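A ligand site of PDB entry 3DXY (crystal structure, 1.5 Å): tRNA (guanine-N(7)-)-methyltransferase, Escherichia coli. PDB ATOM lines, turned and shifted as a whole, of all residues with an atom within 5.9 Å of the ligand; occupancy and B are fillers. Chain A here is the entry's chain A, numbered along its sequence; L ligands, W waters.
A nitrogen (N1) of the ligand lies within hydrogen-bond range of the backbone carbonyl oxygen (O) of Gly 42, 2.8 Å away.
OD1 of Asp 92 sits at hydrogen-bond distance from N4 of the ligand (3.5 Å).
The backbone carbonyl oxygen of Phe 112 lies within hydrogen-bond range of a nitrogen (N1) of the ligand (2.8 Å).
A nitrogen (N5) of the ligand is in hydrogen-bond range of the backbone NH (N) of Ala 93 (3.0 Å).
OE2 of Glu 40 lies within salt-bridge range of N1 of the ligand, at 3.8 Å.
O5 of the ligand is in hydrogen-bond range of OE2 of Glu 65, 2.6 Å away.
The backbone carbonyl oxygen of Phe 113 lies close to a sulfur (S1) of the ligand.
Phe 43 touches the ligand (O to C1, 3.6 Å).
Gly 44 touches the ligand (CA to C3, 3.6 Å).
Ile 64 touches the ligand (CG2 to C14, 3.9 Å).
CG2 of Val 66 touches O5 of the ligand, at 3.6 Å.
His 67 touches the ligand.
Asp 115 touches the ligand.
Hydrophobic or aromatic side chains within 4 Å of the ligand: Ile 64, Val 66, His 67, Ala 93 and Phe 113.
Of the 22 residues printed, 13 come within 4 Å of the ligand.
Water W6 lies within hydrogen-bond range of O2 of the ligand (2.6 Å) and N of Met 45 (2.9 Å).
Water W2 lies within hydrogen-bond range of OE2 of Glu 40 (2.7 Å) and N1 of the ligand (2.8 Å).
Water W12 lies within hydrogen-bond range of the side-chain carboxylate of Asp 92 (2.6 Å) and a nitrogen (N4) of the ligand (3.5 Å).
OE1 of Glu 65 lies within hydrogen-bond range of N of Gly 44 (2.7 Å).
The side-chain carboxylate (OE2) of Glu 65 is in hydrogen-bond range of the backbone NH (N) of His 67 (2.8 Å).
The backbone NH (N) of Phe 43 sits at hydrogen-bond distance from the side-chain carboxylate (OE1) of Glu 65 (3.3 Å).
The backbone carbonyl oxygen (O) of Glu 40 is in hydrogen-bond range of the backbone NH (N) of Ile 64 (2.9 Å).
N of Phe 43 lies within hydrogen-bond range of O of Ile 64, at 3.5 Å.
N of Gly 42 is in hydrogen-bond range of O of Ile 64 (2.7 Å).
The side-chain carboxylate of Asp 92 is in hydrogen-bond range of the backbone NH of Val 94.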
ATOM      1  N   GLU A  40       7.235 -26.395 -27.608  1.00  0.00           N
ATOM      2  CA  GLU A  40       7.425 -25.785 -26.288  1.00  0.00           C
ATOM      3  C   GLU A  40       8.685 -24.947 -26.269  1.00  0.00           C
ATOM      4  O   GLU A  40       9.777 -25.450 -26.566  1.00  0.00           O
ATOM      5  CB  GLU A  40       7.470 -26.808 -25.149  1.00  0.00           C
ATOM      6  CG  GLU A  40       7.583 -26.067 -23.815  1.00  0.00           C
ATOM      7  CD  GLU A  40       7.652 -26.934 -22.590  1.00  0.00           C
ATOM      8  OE1 GLU A  40       7.606 -28.174 -22.711  1.00  0.00           O
ATOM      9  OE2 GLU A  40       7.740 -26.350 -21.487  1.00  0.00           O
ATOM     10  N   ILE A  41       8.539 -23.660 -25.956  1.00  0.00           N
ATOM     11  CA  ILE A  41       9.661 -22.747 -25.892  1.00  0.00           C
ATOM     12  C   ILE A  41      10.158 -22.646 -24.454  1.00  0.00           C
ATOM     13  O   ILE A  41       9.354 -22.369 -23.560  1.00  0.00           O
ATOM     14  CB  ILE A  41       9.259 -21.342 -26.405  1.00  0.00           C
ATOM     15  CG1 ILE A  41       8.941 -21.414 -27.900  1.00  0.00           C
ATOM     16  CG2 ILE A  41      10.350 -20.311 -26.110  1.00  0.00           C
ATOM     17  CD1 ILE A  41       8.272 -20.182 -28.440  1.00  0.00           C
ATOM     18  N   GLY A  42      11.456 -22.857 -24.245  1.00  0.00           N
ATOM     19  CA  GLY A  42      12.034 -22.779 -22.901  1.00  0.00           C
ATOM     20  C   GLY A  42      11.539 -23.905 -22.012  1.00  0.00           C
ATOM     21  O   GLY A  42      11.067 -23.660 -20.893  1.00  0.00           O
ATOM     22  N   PHE A  43      11.694 -25.139 -22.489  1.00  0.00           N
ATOM     23  CA  PHE A  43      11.149 -26.307 -21.792  1.00  0.00           C
ATOM     24  C   PHE A  43      11.859 -26.673 -20.488  1.00  0.00           C
ATOM     25  O   PHE A  43      11.401 -27.571 -19.775  1.00  0.00           O
ATOM     26  CB  PHE A  43      11.046 -27.505 -22.733  1.00  0.00           C
ATOM     27  CG  PHE A  43      12.358 -27.971 -23.288  1.00  0.00           C
ATOM     28  CD1 PHE A  43      13.282 -28.629 -22.487  1.00  0.00           C
ATOM     29  CD2 PHE A  43      12.654 -27.811 -24.632  1.00  0.00           C
ATOM     30  CE1 PHE A  43      14.497 -29.089 -23.015  1.00  0.00           C
ATOM     31  CE2 PHE A  43      13.854 -28.268 -25.172  1.00  0.00           C
ATOM     32  CZ  PHE A  43      14.779 -28.906 -24.367  1.00  0.00           C
ATOM     33  N   GLY A  44      12.972 -26.008 -20.204  1.00  0.00           N
ATOM     34  CA  GLY A  44      13.736 -26.277 -18.980  1.00  0.00           C
ATOM     35  C   GLY A  44      14.313 -27.682 -19.002  1.00  0.00           C
ATOM     36  O   GLY A  44      15.058 -28.034 -19.919  1.00  0.00           O
ATOM     37  N   MET A  45      13.958 -28.485 -18.006  1.00  0.00           N
ATOM     38  CA  MET A  45      14.416 -29.862 -17.951  1.00  0.00           C
ATOM     39  C   MET A  45      13.496 -30.798 -18.739  1.00  0.00           C
ATOM     40  O   MET A  45      13.746 -32.010 -18.823  1.00  0.00           O
ATOM     41  CB  MET A  45      14.587 -30.317 -16.502  1.00  0.00           C
ATOM     42  CG  MET A  45      15.818 -29.696 -15.855  1.00  0.00           C
ATOM     43  SD  MET A  45      15.865 -29.811 -14.055  1.00  0.00           S
ATOM     44  CE  MET A  45      15.733 -31.581 -13.809  1.00  0.00           C
ATOM     45  N   ILE A  64      12.404 -26.158 -27.580  1.00  0.00           N
ATOM     46  CA  ILE A  64      13.582 -25.308 -27.716  1.00  0.00           C
ATOM     47  C   ILE A  64      14.028 -24.859 -26.333  1.00  0.00           C
ATOM     48  O   ILE A  64      13.198 -24.407 -25.546  1.00  0.00           O
ATOM     49  CB  ILE A  64      13.298 -24.062 -28.565  1.00  0.00           C
ATOM     50  CG1 ILE A  64      12.753 -24.451 -29.938  1.00  0.00           C
ATOM     51  CG2 ILE A  64      14.576 -23.245 -28.704  1.00  0.00           C
ATOM     52  CD1 ILE A  64      12.154 -23.271 -30.678  1.00  0.00           C
ATOM     53  N   GLU A  65      15.320 -24.982 -26.047  1.00  0.00           N
ATOM     54  CA  GLU A  65      15.824 -24.572 -24.729  1.00  0.00           C
ATOM     55  C   GLU A  65      17.292 -24.235 -24.828  1.00  0.00           C
ATOM     56  O   GLU A  65      18.091 -25.103 -25.209  1.00  0.00           O
ATOM     57  CB  GLU A  65      15.592 -25.707 -23.720  1.00  0.00           C
ATOM     58  CG  GLU A  65      16.085 -25.519 -22.308  1.00  0.00           C
ATOM     59  CD  GLU A  65      15.683 -24.176 -21.738  1.00  0.00           C
ATOM     60  OE1 GLU A  65      14.534 -24.033 -21.267  1.00  0.00           O
ATOM     61  OE2 GLU A  65      16.550 -23.288 -21.730  1.00  0.00           O
ATOM     62  N   VAL A  66      17.649 -22.996 -24.480  1.00  0.00           N
ATOM     63  CA  VAL A  66      19.046 -22.536 -24.575  1.00  0.00           C
ATOM     64  C   VAL A  66      19.919 -22.982 -23.399  1.00  0.00           C
ATOM     65  O   VAL A  66      21.151 -22.833 -23.451  1.00  0.00           O
ATOM     66  CB  VAL A  66      19.163 -20.993 -24.705  1.00  0.00           C
ATOM     67  CG1 VAL A  66      18.721 -20.535 -26.087  1.00  0.00           C
ATOM     68  CG2 VAL A  66      18.388 -20.267 -23.615  1.00  0.00           C
ATOM     69  N   HIS A  67      19.313 -23.516 -22.350  1.00  0.00           N
ATOM     70  CA  HIS A  67      20.065 -23.977 -21.185  1.00  0.00           C
ATOM     71  C   HIS A  67      20.409 -25.431 -21.445  1.00  0.00           C
ATOM     72  O   HIS A  67      19.555 -26.313 -21.337  1.00  0.00           O
ATOM     73  CB  HIS A  67      19.219 -23.785 -19.911  1.00  0.00           C
ATOM     74  CG  HIS A  67      19.896 -24.215 -18.645  1.00  0.00           C
ATOM     75  ND1 HIS A  67      21.071 -23.647 -18.184  1.00  0.00           N
ATOM     76  CD2 HIS A  67      19.520 -25.108 -17.708  1.00  0.00           C
ATOM     77  CE1 HIS A  67      21.402 -24.210 -17.029  1.00  0.00           C
ATOM     78  NE2 HIS A  67      20.478 -25.100 -16.719  1.00  0.00           N
ATOM     79  N   HIS A  91      18.972 -23.461 -29.035  1.00  0.00           N
ATOM     80  CA  HIS A  91      19.210 -22.252 -29.805  1.00  0.00           C
ATOM     81  C   HIS A  91      18.147 -21.244 -29.431  1.00  0.00           C
ATOM     82  O   HIS A  91      17.049 -21.631 -29.015  1.00  0.00           O
ATOM     83  CB  HIS A  91      19.127 -22.533 -31.304  1.00  0.00           C
ATOM     84  CG  HIS A  91      19.798 -21.502 -32.145  1.00  0.00           C
ATOM     85  ND1 HIS A  91      19.153 -20.367 -32.605  1.00  0.00           N
ATOM     86  CD2 HIS A  91      21.079 -21.400 -32.581  1.00  0.00           C
ATOM     87  CE1 HIS A  91      20.005 -19.633 -33.301  1.00  0.00           C
ATOM     88  NE2 HIS A  91      21.173 -20.247 -33.310  1.00  0.00           N
ATOM     89  N   ASP A  92      18.454 -19.965 -29.585  1.00  0.00           N
ATOM     90  CA  ASP A  92      17.499 -18.888 -29.318  1.00  0.00           C
ATOM     91  C   ASP A  92      16.182 -19.179 -30.026  1.00  0.00           C
ATOM     92  O   ASP A  92      16.158 -19.291 -31.251  1.00  0.00           O
ATOM     93  CB  ASP A  92      18.086 -17.562 -29.836  1.00  0.00           C
ATOM     94  CG  ASP A  92      17.145 -16.391 -29.631  1.00  0.00           C
ATOM     95  OD1 ASP A  92      17.162 -15.816 -28.523  1.00  0.00           O
ATOM     96  OD2 ASP A  92      16.417 -16.042 -30.589  1.00  0.00           O
ATOM     97  N   ALA A  93      15.094 -19.288 -29.264  1.00  0.00           N
ATOM     98  CA  ALA A  93      13.792 -19.617 -29.836  1.00  0.00           C
ATOM     99  C   ALA A  93      13.289 -18.606 -30.867  1.00  0.00           C
ATOM    100  O   ALA A  93      12.601 -18.986 -31.810  1.00  0.00           O
ATOM    101  CB  ALA A  93      12.749 -19.804 -28.740  1.00  0.00           C
ATOM    102  N   VAL A  94      13.607 -17.335 -30.676  1.00  0.00           N
ATOM    103  CA  VAL A  94      13.150 -16.322 -31.618  1.00  0.00           C
ATOM    104  C   VAL A  94      13.806 -16.520 -32.995  1.00  0.00           C
ATOM    105  O   VAL A  94      13.135 -16.464 -34.025  1.00  0.00           O
ATOM    106  CB  VAL A  94      13.372 -14.895 -31.072  1.00  0.00           C
ATOM    107  CG1 VAL A  94      13.016 -13.843 -32.119  1.00  0.00           C
ATOM    108  CG2 VAL A  94      12.526 -14.704 -29.798  1.00  0.00           C
ATOM    109  N   PHE A 112       5.969 -21.982 -20.762  1.00  0.00           N
ATOM    110  CA  PHE A 112       5.666 -22.165 -19.349  1.00  0.00           C
ATOM    111  C   PHE A 112       6.758 -21.604 -18.489  1.00  0.00           C
ATOM    112  O   PHE A 112       7.926 -21.971 -18.608  1.00  0.00           O
ATOM    113  CB  PHE A 112       5.455 -23.651 -19.037  1.00  0.00           C
ATOM    114  CG  PHE A 112       4.304 -24.284 -19.789  1.00  0.00           C
ATOM    115  CD1 PHE A 112       3.221 -23.511 -20.229  1.00  0.00           C
ATOM    116  CD2 PHE A 112       4.302 -25.654 -20.029  1.00  0.00           C
ATOM    117  CE1 PHE A 112       2.164 -24.108 -20.912  1.00  0.00           C
ATOM    118  CE2 PHE A 112       3.246 -26.254 -20.698  1.00  0.00           C
ATOM    119  CZ  PHE A 112       2.185 -25.482 -21.134  1.00  0.00           C
ATOM    120  N   PHE A 113       6.373 -20.694 -17.594  1.00  0.00           N
ATOM    121  CA  PHE A 113       7.299 -20.038 -16.681  1.00  0.00           C
ATOM    122  C   PHE A 113       8.486 -19.392 -17.382  1.00  0.00           C
ATOM    123  O   PHE A 113       9.633 -19.584 -16.992  1.00  0.00           O
ATOM    124  CB  PHE A 113       7.705 -21.003 -15.565  1.00  0.00           C
ATOM    125  CG  PHE A 113       6.526 -21.615 -14.930  1.00  0.00           C
ATOM    126  CD1 PHE A 113       5.771 -20.892 -14.032  1.00  0.00           C
ATOM    127  CD2 PHE A 113       6.079 -22.876 -15.315  1.00  0.00           C
ATOM    128  CE1 PHE A 113       4.626 -21.419 -13.471  1.00  0.00           C
ATOM    129  CE2 PHE A 113       4.934 -23.422 -14.759  1.00  0.00           C
ATOM    130  CZ  PHE A 113       4.211 -22.685 -13.832  1.00  0.00           C
ATOM    131  N   PRO A 114       8.196 -18.577 -18.419  1.00  0.00           N
ATOM    132  CA  PRO A 114       9.300 -17.846 -19.028  1.00  0.00           C
ATOM    133  C   PRO A 114       9.920 -16.903 -17.986  1.00  0.00           C
ATOM    134  O   PRO A 114       9.227 -16.484 -17.054  1.00  0.00           O
ATOM    135  CB  PRO A 114       8.626 -17.031 -20.130  1.00  0.00           C
ATOM    136  CG  PRO A 114       7.198 -16.931 -19.723  1.00  0.00           C
ATOM    137  CD  PRO A 114       6.890 -18.229 -19.014  1.00  0.00           C
ATOM    138  N   ASP A 115      11.204 -16.591 -18.148  1.00  0.00           N
ATOM    139  CA  ASP A 115      11.931 -15.780 -17.175  1.00  0.00           C
ATOM    140  C   ASP A 115      11.089 -14.565 -16.791  1.00  0.00           C
ATOM    141  O   ASP A 115      10.728 -13.766 -17.641  1.00  0.00           O
ATOM    142  CB  ASP A 115      13.279 -15.332 -17.767  1.00  0.00           C
ATOM    143  CG  ASP A 115      14.124 -16.499 -18.243  1.00  0.00           C
ATOM    144  OD1 ASP A 115      14.015 -17.602 -17.662  1.00  0.00           O
ATOM    145  OD2 ASP A 115      14.929 -16.308 -19.181  1.00  0.00           O
ATOM    146  N   PRO A 116      10.714 -14.457 -15.500  1.00  0.00           N
ATOM    147  CA  PRO A 116       9.768 -13.416 -15.103  1.00  0.00           C
ATOM    148  C   PRO A 116      10.342 -12.027 -14.968  1.00  0.00           C
ATOM    149  O   PRO A 116       9.574 -11.057 -14.947  1.00  0.00           O
ATOM    150  CB  PRO A 116       9.252 -13.919 -13.753  1.00  0.00           C
ATOM    151  CG  PRO A 116      10.391 -14.675 -13.199  1.00  0.00           C
ATOM    152  CD  PRO A 116      11.056 -15.350 -14.383  1.00  0.00           C
ATOM    153  N   ILE A 127      10.089 -12.179 -22.518  1.00  0.00           N
ATOM    154  CA  ILE A 127       9.955 -12.604 -23.902  1.00  0.00           C
ATOM    155  C   ILE A 127       8.568 -12.271 -24.462  1.00  0.00           C
ATOM    156  O   ILE A 127       8.432 -12.019 -25.659  1.00  0.00           O
ATOM    157  CB  ILE A 127      10.294 -14.095 -24.081  1.00  0.00           C
ATOM    158  CG1 ILE A 127      10.585 -14.431 -25.547  1.00  0.00           C
ATOM    159  CG2 ILE A 127       9.199 -15.010 -23.525  1.00  0.00           C
ATOM    160  CD1 ILE A 127      11.212 -15.809 -25.757  1.00  0.00           C
ATOM    161  N   THR A 188       2.707 -27.665 -10.797  1.00  0.00           N
ATOM    162  CA  THR A 188       4.061 -27.387 -10.336  1.00  0.00           C
ATOM    163  C   THR A 188       4.087 -27.126  -8.834  1.00  0.00           C
ATOM    164  O   THR A 188       3.043 -26.989  -8.188  1.00  0.00           O
ATOM    165  CB  THR A 188       4.644 -26.132 -11.012  1.00  0.00           C
ATOM    166  OG1 THR A 188       3.990 -24.962 -10.470  1.00  0.00           O
ATOM    167  CG2 THR A 188       4.459 -26.183 -12.526  1.00  0.00           C
ATOM    168  N   PHE A 190       4.977 -24.429  -7.513  1.00  0.00           N
ATOM    169  CA  PHE A 190       4.638 -23.020  -7.336  1.00  0.00           C
ATOM    170  C   PHE A 190       3.143 -22.865  -7.092  1.00  0.00           C
ATOM    171  O   PHE A 190       2.648 -21.751  -6.848  1.00  0.00           O
ATOM    172  CB  PHE A 190       5.074 -22.212  -8.565  1.00  0.00           C
ATOM    173  CG  PHE A 190       6.478 -22.471  -8.994  1.00  0.00           C
ATOM    174  CD1 PHE A 190       6.741 -23.101 -10.210  1.00  0.00           C
ATOM    175  CD2 PHE A 190       7.558 -22.115  -8.181  1.00  0.00           C
ATOM    176  CE1 PHE A 190       8.056 -23.364 -10.608  1.00  0.00           C
ATOM    177  CE2 PHE A 190       8.873 -22.368  -8.577  1.00  0.00           C
ATOM    178  CZ  PHE A 190       9.122 -22.998  -9.791  1.00  0.00           C
HETATM  179  N1  LIG L   1       9.393 -24.366 -18.713  1.00  0.00           N
HETATM  180  C1  LIG L   1      10.444 -24.798 -17.729  1.00  0.00           C
HETATM  181  C2  LIG L   1       9.837 -25.027 -16.363  1.00  0.00           C
HETATM  182  O1  LIG L   1       8.688 -24.622 -16.130  1.00  0.00           O
HETATM  183  O2  LIG L   1      10.459 -25.596 -15.467  1.00  0.00           O
HETATM  184  C3  LIG L   1      11.549 -23.759 -17.630  1.00  0.00           C
HETATM  185  C4  LIG L   1      11.160 -22.448 -16.951  1.00  0.00           C
HETATM  186  S1  LIG L   1      12.618 -21.407 -16.747  1.00  0.00           S
HETATM  187  C5  LIG L   1      12.066 -20.218 -15.494  1.00  0.00           C
HETATM  188  C6  LIG L   1      12.606 -20.447 -18.286  1.00  0.00           C
HETATM  189  C7  LIG L   1      13.403 -21.155 -19.368  1.00  0.00           C
HETATM  190  O3  LIG L   1      13.324 -20.416 -20.560  1.00  0.00           O
HETATM  191  C8  LIG L   1      14.886 -21.263 -19.028  1.00  0.00           C
HETATM  192  O4  LIG L   1      15.252 -22.636 -19.034  1.00  0.00           O
HETATM  193  C9  LIG L   1      15.600 -20.487 -20.128  1.00  0.00           C
HETATM  194  O5  LIG L   1      16.839 -21.057 -20.514  1.00  0.00           O
HETATM  195  C10 LIG L   1      14.558 -20.551 -21.235  1.00  0.00           C
HETATM  196  N2  LIG L   1      14.664 -19.478 -22.229  1.00  0.00           N
HETATM  197  C11 LIG L   1      14.670 -18.134 -22.016  1.00  0.00           C
HETATM  198  N3  LIG L   1      14.777 -17.511 -23.209  1.00  0.00           N
HETATM  199  C12 LIG L   1      14.811 -18.449 -24.186  1.00  0.00           C
HETATM  200  C13 LIG L   1      14.918 -18.350 -25.564  1.00  0.00           C
HETATM  201  N4  LIG L   1      14.988 -17.166 -26.190  1.00  0.00           N
HETATM  202  N5  LIG L   1      14.945 -19.509 -26.302  1.00  0.00           N
HETATM  203  C14 LIG L   1      14.861 -20.742 -25.684  1.00  0.00           C
HETATM  204  N6  LIG L   1      14.767 -20.841 -24.308  1.00  0.00           N
HETATM  205  C15 LIG L   1      14.740 -19.701 -23.574  1.00  0.00           C
HETATM  206  O   HOH W   1       7.579 -25.886 -14.386  1.00  0.00           O
HETATM  207  O   HOH W   2       7.818 -26.666 -18.838  1.00  0.00           O
HETATM  208  O   HOH W   3      15.308 -14.589 -24.872  1.00  0.00           O
HETATM  209  O   HOH W   4      11.172 -18.951 -21.756  1.00  0.00           O
HETATM  210  O   HOH W   5       7.968 -23.679 -21.555  1.00  0.00           O
HETATM  211  O   HOH W   6      12.504 -27.202 -15.855  1.00  0.00           O
HETATM  212  O   HOH W   7      19.514 -20.048 -20.120  1.00  0.00           O
HETATM  213  O   HOH W   8      16.583 -24.939 -17.748  1.00  0.00           O
HETATM  214  O   HOH W   9       6.075 -26.060 -16.683  1.00  0.00           O
HETATM  215  O   HOH W  10      13.660 -14.934 -22.774  1.00  0.00           O
HETATM  216  O   HOH W  11      10.894 -18.714 -12.735  1.00  0.00           O
HETATM  217  O   HOH W  12      15.579 -13.990 -27.445  1.00  0.00           O
